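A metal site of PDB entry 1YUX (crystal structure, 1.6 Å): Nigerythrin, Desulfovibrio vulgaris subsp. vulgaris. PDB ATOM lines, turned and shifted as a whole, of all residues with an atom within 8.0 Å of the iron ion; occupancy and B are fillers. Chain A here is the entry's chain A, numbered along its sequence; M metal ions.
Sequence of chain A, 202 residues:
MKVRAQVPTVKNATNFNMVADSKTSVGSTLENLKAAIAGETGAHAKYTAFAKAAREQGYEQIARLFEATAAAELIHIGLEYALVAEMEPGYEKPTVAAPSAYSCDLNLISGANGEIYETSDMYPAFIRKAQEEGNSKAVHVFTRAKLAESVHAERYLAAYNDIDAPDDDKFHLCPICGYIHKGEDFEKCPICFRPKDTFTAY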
ATOM      1  N   ILE A  75     -24.144   4.593 -17.780  1.00  0.00           N
ATOM      2  CA  ILE A  75     -23.548   5.785 -18.370  1.00  0.00           C
ATOM      3  C   ILE A  75     -23.313   5.464 -19.851  1.00  0.00           C
ATOM      4  O   ILE A  75     -23.602   6.280 -20.724  1.00  0.00           O
ATOM      5  CB  ILE A  75     -22.205   6.140 -17.691  1.00  0.00           C
ATOM      6  CG1 ILE A  75     -22.475   6.718 -16.297  1.00  0.00           C
ATOM      7  CG2 ILE A  75     -21.425   7.140 -18.548  1.00  0.00           C
ATOM      8  CD1 ILE A  75     -21.217   7.018 -15.506  1.00  0.00           C
ATOM      9  N   ARG A 144     -14.898   5.513 -25.802  1.00  0.00           N
ATOM     10  CA  ARG A 144     -15.027   5.796 -24.384  1.00  0.00           C
ATOM     11  C   ARG A 144     -15.488   4.560 -23.626  1.00  0.00           C
ATOM     12  O   ARG A 144     -14.924   4.216 -22.589  1.00  0.00           O
ATOM     13  CB  ARG A 144     -16.020   6.953 -24.182  1.00  0.00           C
ATOM     14  CG  ARG A 144     -16.129   7.442 -22.754  1.00  0.00           C
ATOM     15  CD  ARG A 144     -16.376   8.944 -22.711  1.00  0.00           C
ATOM     16  NE  ARG A 144     -15.213   9.695 -23.177  1.00  0.00           N
ATOM     17  CZ  ARG A 144     -15.091  11.014 -23.121  1.00  0.00           C
ATOM     18  NH1 ARG A 144     -16.083  11.755 -22.627  1.00  0.00           N
ATOM     19  NH2 ARG A 144     -13.984  11.604 -23.548  1.00  0.00           N
ATOM     20  N   ALA A 148     -13.352   1.930 -20.772  1.00  0.00           N
ATOM     21  CA  ALA A 148     -13.837   1.662 -19.436  1.00  0.00           C
ATOM     22  C   ALA A 148     -13.968   0.163 -19.151  1.00  0.00           C
ATOM     23  O   ALA A 148     -13.714  -0.289 -18.034  1.00  0.00           O
ATOM     24  CB  ALA A 148     -15.186   2.337 -19.220  1.00  0.00           C
ATOM     25  N   LEU A 173     -16.800   6.463  -9.414  1.00  0.00           N
ATOM     26  CA  LEU A 173     -17.221   6.399 -10.809  1.00  0.00           C
ATOM     27  C   LEU A 173     -17.209   7.775 -11.449  1.00  0.00           C
ATOM     28  O   LEU A 173     -17.707   8.747 -10.872  1.00  0.00           O
ATOM     29  CB  LEU A 173     -18.636   5.815 -10.892  1.00  0.00           C
ATOM     30  CG  LEU A 173     -19.276   5.737 -12.281  1.00  0.00           C
ATOM     31  CD1 LEU A 173     -18.440   4.818 -13.171  1.00  0.00           C
ATOM     32  CD2 LEU A 173     -20.697   5.223 -12.149  1.00  0.00           C
ATOM     33  N   CYS A 174     -16.636   7.850 -12.643  1.00  0.00           N
ATOM     34  CA  CYS A 174     -16.569   9.102 -13.394  1.00  0.00           C
ATOM     35  C   CYS A 174     -17.991   9.524 -13.776  1.00  0.00           C
ATOM     36  O   CYS A 174     -18.843   8.684 -13.997  1.00  0.00           O
ATOM     37  CB  CYS A 174     -15.717   8.898 -14.652  1.00  0.00           C
ATOM     38  SG  CYS A 174     -15.627  10.351 -15.728  1.00  0.00           S
ATOM     39  N   PRO A 175     -18.241  10.836 -13.854  1.00  0.00           N
ATOM     40  CA  PRO A 175     -19.575  11.327 -14.218  1.00  0.00           C
ATOM     41  C   PRO A 175     -19.998  11.135 -15.665  1.00  0.00           C
ATOM     42  O   PRO A 175     -21.190  10.995 -15.952  1.00  0.00           O
ATOM     43  CB  PRO A 175     -19.509  12.803 -13.830  1.00  0.00           C
ATOM     44  CG  PRO A 175     -18.072  13.151 -14.075  1.00  0.00           C
ATOM     45  CD  PRO A 175     -17.353  11.959 -13.477  1.00  0.00           C
ATOM     46  N   ILE A 176     -19.034  11.099 -16.584  1.00  0.00           N
ATOM     47  CA  ILE A 176     -19.366  10.958 -17.991  1.00  0.00           C
ATOM     48  C   ILE A 176     -18.833   9.729 -18.730  1.00  0.00           C
ATOM     49  O   ILE A 176     -19.119   9.548 -19.917  1.00  0.00           O
ATOM     50  CB  ILE A 176     -18.963  12.227 -18.779  1.00  0.00           C
ATOM     51  CG1 ILE A 176     -17.449  12.409 -18.720  1.00  0.00           C
ATOM     52  CG2 ILE A 176     -19.670  13.444 -18.175  1.00  0.00           C
ATOM     53  CD1 ILE A 176     -16.935  13.575 -19.562  1.00  0.00           C
ATOM     54  N   CYS A 177     -18.055   8.902 -18.048  1.00  0.00           N
ATOM     55  CA  CYS A 177     -17.552   7.677 -18.670  1.00  0.00           C
ATOM     56  C   CYS A 177     -17.570   6.588 -17.614  1.00  0.00           C
ATOM     57  O   CYS A 177     -17.819   6.859 -16.433  1.00  0.00           O
ATOM     58  CB  CYS A 177     -16.142   7.879 -19.264  1.00  0.00           C
ATOM     59  SG  CYS A 177     -14.732   7.654 -18.170  1.00  0.00           S
ATOM     60  N   GLY A 178     -17.312   5.350 -18.021  1.00  0.00           N
ATOM     61  CA  GLY A 178     -17.362   4.241 -17.080  1.00  0.00           C
ATOM     62  C   GLY A 178     -16.153   4.001 -16.204  1.00  0.00           C
ATOM     63  O   GLY A 178     -16.082   2.986 -15.514  1.00  0.00           O
ATOM     64  N   TYR A 179     -15.201   4.925 -16.203  1.00  0.00           N
ATOM     65  CA  TYR A 179     -14.011   4.730 -15.390  1.00  0.00           C
ATOM     66  C   TYR A 179     -14.327   4.608 -13.907  1.00  0.00           C
ATOM     67  O   TYR A 179     -15.120   5.380 -13.367  1.00  0.00           O
ATOM     68  CB  TYR A 179     -13.031   5.884 -15.590  1.00  0.00           C
ATOM     69  CG  TYR A 179     -11.812   5.762 -14.711  1.00  0.00           C
ATOM     70  CD1 TYR A 179     -10.858   4.778 -14.939  1.00  0.00           C
ATOM     71  CD2 TYR A 179     -11.629   6.630 -13.632  1.00  0.00           C
ATOM     72  CE1 TYR A 179      -9.743   4.648 -14.109  1.00  0.00           C
ATOM     73  CE2 TYR A 179     -10.526   6.504 -12.797  1.00  0.00           C
ATOM     74  CZ  TYR A 179      -9.585   5.529 -13.044  1.00  0.00           C
ATOM     75  OH  TYR A 179      -8.480   5.428 -12.225  1.00  0.00           O
ATOM     76  N   ILE A 180     -13.702   3.639 -13.259  1.00  0.00           N
ATOM     77  CA  ILE A 180     -13.888   3.403 -11.833  1.00  0.00           C
ATOM     78  C   ILE A 180     -12.524   3.293 -11.175  1.00  0.00           C
ATOM     79  O   ILE A 180     -11.648   2.583 -11.664  1.00  0.00           O
ATOM     80  CB  ILE A 180     -14.645   2.090 -11.563  1.00  0.00           C
ATOM     81  CG1 ILE A 180     -16.091   2.226 -12.032  1.00  0.00           C
ATOM     82  CG2 ILE A 180     -14.596   1.734 -10.072  1.00  0.00           C
ATOM     83  CD1 ILE A 180     -16.864   0.921 -12.022  1.00  0.00           C
ATOM     84  N   LYS A 188      -7.611  12.546 -11.513  1.00  0.00           N
ATOM     85  CA  LYS A 188      -8.631  12.707 -12.544  1.00  0.00           C
ATOM     86  C   LYS A 188      -8.814  11.431 -13.341  1.00  0.00           C
ATOM     87  O   LYS A 188      -8.017  10.501 -13.238  1.00  0.00           O
ATOM     88  CB  LYS A 188      -8.247  13.847 -13.483  1.00  0.00           C
ATOM     89  CG  LYS A 188      -6.942  13.609 -14.227  1.00  0.00           C
ATOM     90  CD  LYS A 188      -6.669  14.714 -15.228  1.00  0.00           C
ATOM     91  CE  LYS A 188      -5.366  14.455 -15.979  1.00  0.00           C
ATOM     92  NZ  LYS A 188      -5.095  15.500 -17.012  1.00  0.00           N
ATOM     93  N   CYS A 189      -9.876  11.405 -14.143  1.00  0.00           N
ATOM     94  CA  CYS A 189     -10.190  10.253 -14.970  1.00  0.00           C
ATOM     95  C   CYS A 189      -9.169  10.126 -16.102  1.00  0.00           C
ATOM     96  O   CYS A 189      -8.932  11.082 -16.834  1.00  0.00           O
ATOM     97  CB  CYS A 189     -11.590  10.402 -15.554  1.00  0.00           C
ATOM     98  SG  CYS A 189     -12.111   9.012 -16.580  1.00  0.00           S
ATOM     99  N   PRO A 190      -8.547   8.942 -16.242  1.00  0.00           N
ATOM    100  CA  PRO A 190      -7.547   8.725 -17.290  1.00  0.00           C
ATOM    101  C   PRO A 190      -8.154   8.544 -18.685  1.00  0.00           C
ATOM    102  O   PRO A 190      -7.434   8.536 -19.690  1.00  0.00           O
ATOM    103  CB  PRO A 190      -6.818   7.476 -16.814  1.00  0.00           C
ATOM    104  CG  PRO A 190      -7.904   6.713 -16.137  1.00  0.00           C
ATOM    105  CD  PRO A 190      -8.629   7.779 -15.351  1.00  0.00           C
ATOM    106  N   ILE A 191      -9.475   8.399 -18.739  1.00  0.00           N
ATOM    107  CA  ILE A 191     -10.170   8.216 -19.995  1.00  0.00           C
ATOM    108  C   ILE A 191     -10.711   9.533 -20.559  1.00  0.00           C
ATOM    109  O   ILE A 191     -10.582   9.791 -21.756  1.00  0.00           O
ATOM    110  CB  ILE A 191     -11.356   7.219 -19.842  1.00  0.00           C
ATOM    111  CG1 ILE A 191     -10.807   5.824 -19.520  1.00  0.00           C
ATOM    112  CG2 ILE A 191     -12.186   7.186 -21.123  1.00  0.00           C
ATOM    113  CD1 ILE A 191     -11.877   4.787 -19.248  1.00  0.00           C
ATOM    114  N   CYS A 192     -11.293  10.369 -19.705  1.00  0.00           N
ATOM    115  CA  CYS A 192     -11.845  11.639 -20.178  1.00  0.00           C
ATOM    116  C   CYS A 192     -11.303  12.867 -19.446  1.00  0.00           C
ATOM    117  O   CYS A 192     -11.669  14.001 -19.768  1.00  0.00           O
ATOM    118  CB  CYS A 192     -13.369  11.626 -20.058  1.00  0.00           C
ATOM    119  SG  CYS A 192     -13.955  11.647 -18.357  1.00  0.00           S
ATOM    120  N   PHE A 193     -10.437  12.647 -18.464  1.00  0.00           N
ATOM    121  CA  PHE A 193      -9.806  13.724 -17.703  1.00  0.00           C
ATOM    122  C   PHE A 193     -10.674  14.471 -16.685  1.00  0.00           C
ATOM    123  O   PHE A 193     -10.226  15.454 -16.090  1.00  0.00           O
ATOM    124  CB  PHE A 193      -9.148  14.723 -18.657  1.00  0.00           C
ATOM    125  CG  PHE A 193      -7.840  14.244 -19.232  1.00  0.00           C
ATOM    126  CD1 PHE A 193      -7.523  12.881 -19.260  1.00  0.00           C
ATOM    127  CD2 PHE A 193      -6.923  15.144 -19.774  1.00  0.00           C
ATOM    128  CE1 PHE A 193      -6.321  12.439 -19.809  1.00  0.00           C
ATOM    129  CE2 PHE A 193      -5.723  14.715 -20.321  1.00  0.00           C
ATOM    130  CZ  PHE A 193      -5.411  13.351 -20.341  1.00  0.00           C
ATOM    131  N   ARG A 194     -11.906  14.017 -16.480  1.00  0.00           N
ATOM    132  CA  ARG A 194     -12.791  14.652 -15.506  1.00  0.00           C
ATOM    133  C   ARG A 194     -12.142  14.645 -14.124  1.00  0.00           C
ATOM    134  O   ARG A 194     -11.585  13.632 -13.698  1.00  0.00           O
ATOM    135  CB  ARG A 194     -14.133  13.937 -15.440  1.00  0.00           C
ATOM    136  CG  ARG A 194     -15.201  14.503 -16.348  1.00  0.00           C
ATOM    137  CD  ARG A 194     -15.613  15.894 -15.877  1.00  0.00           C
ATOM    138  NE  ARG A 194     -16.787  16.387 -16.593  1.00  0.00           N
ATOM    139  CZ  ARG A 194     -16.795  16.775 -17.859  1.00  0.00           C
ATOM    140  NH1 ARG A 194     -15.675  16.743 -18.583  1.00  0.00           N
ATOM    141  NH2 ARG A 194     -17.919  17.204 -18.421  1.00  0.00           N
ATOM    142  N   PRO A 195     -12.188  15.783 -13.412  1.00  0.00           N
ATOM    143  CA  PRO A 195     -11.599  15.891 -12.075  1.00  0.00           C
ATOM    144  C   PRO A 195     -12.235  14.938 -11.068  1.00  0.00           C
ATOM    145  O   PRO A 195     -13.415  14.605 -11.166  1.00  0.00           O
ATOM    146  CB  PRO A 195     -11.833  17.345 -11.714  1.00  0.00           C
ATOM    147  CG  PRO A 195     -11.801  18.033 -13.040  1.00  0.00           C
ATOM    148  CD  PRO A 195     -12.635  17.098 -13.887  1.00  0.00           C
ATOM    149  N   THR A 198     -15.712  15.374  -9.328  1.00  0.00           N
ATOM    150  CA  THR A 198     -16.954  15.238 -10.087  1.00  0.00           C
ATOM    151  C   THR A 198     -17.454  13.790 -10.091  1.00  0.00           C
ATOM    152  O   THR A 198     -18.521  13.497 -10.624  1.00  0.00           O
ATOM    153  CB  THR A 198     -16.781  15.703 -11.543  1.00  0.00           C
ATOM    154  OG1 THR A 198     -15.893  14.815 -12.238  1.00  0.00           O
ATOM    155  CG2 THR A 198     -16.211  17.112 -11.589  1.00  0.00           C
ATOM    156  N   PHE A 199     -16.678  12.903  -9.477  1.00  0.00           N
ATOM    157  CA  PHE A 199     -17.020  11.493  -9.387  1.00  0.00           C
ATOM    158  C   PHE A 199     -18.087  11.220  -8.341  1.00  0.00           C
ATOM    159  O   PHE A 199     -18.428  12.080  -7.526  1.00  0.00           O
ATOM    160  CB  PHE A 199     -15.773  10.669  -9.030  1.00  0.00           C
ATOM    161  CG  PHE A 199     -14.831  10.409 -10.180  1.00  0.00           C
ATOM    162  CD1 PHE A 199     -14.357  11.456 -10.959  1.00  0.00           C
ATOM    163  CD2 PHE A 199     -14.389   9.118 -10.451  1.00  0.00           C
ATOM    164  CE1 PHE A 199     -13.447  11.213 -11.989  1.00  0.00           C
ATOM    165  CE2 PHE A 199     -13.490   8.866 -11.478  1.00  0.00           C
ATOM    166  CZ  PHE A 199     -13.011   9.920 -12.252  1.00  0.00           C
HETATM  167 FE    FE M   1     -14.171   9.672 -17.321  1.00  0.00          FE
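The backbone NH of Arg 194 sits close to the side-chain sulfur of Cys 192 (3.7 Å). SG of Cys 177 lies close to N of Tyr 179, 3.4 Å away. The backbone NH (N) of Cys 174 is in hydrogen-bond range of the backbone carbonyl oxygen (O) of Tyr 179 (3.0 Å). The side-chain sulfur of Cys 174 lies close to the backbone NH of Ile 176 (3.6 Å). The backbone NH (N) of Ile 191 sits close to the side-chain sulfur (SG) of Cys 189, at 3.5 Å. The backbone carbonyl oxygen (O) of Arg 194 is in hydrogen-bond range of the backbone NH (N) of Cys 189, 2.8 Å away.
Four residues have an atom within 4 Å of the iron ion: Cys 174, Cys 177, Cys 189 and Cys 192. The nearest printed residue that does not touch the iron ion is Tyr 179 (4.3 Å).
The iron ion is bound by SG of Cys 192 (2.2 Å), SG of Cys 177 (2.3 Å), SG of Cys 174 (2.3 Å) and SG of Cys 189 (2.3 Å).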
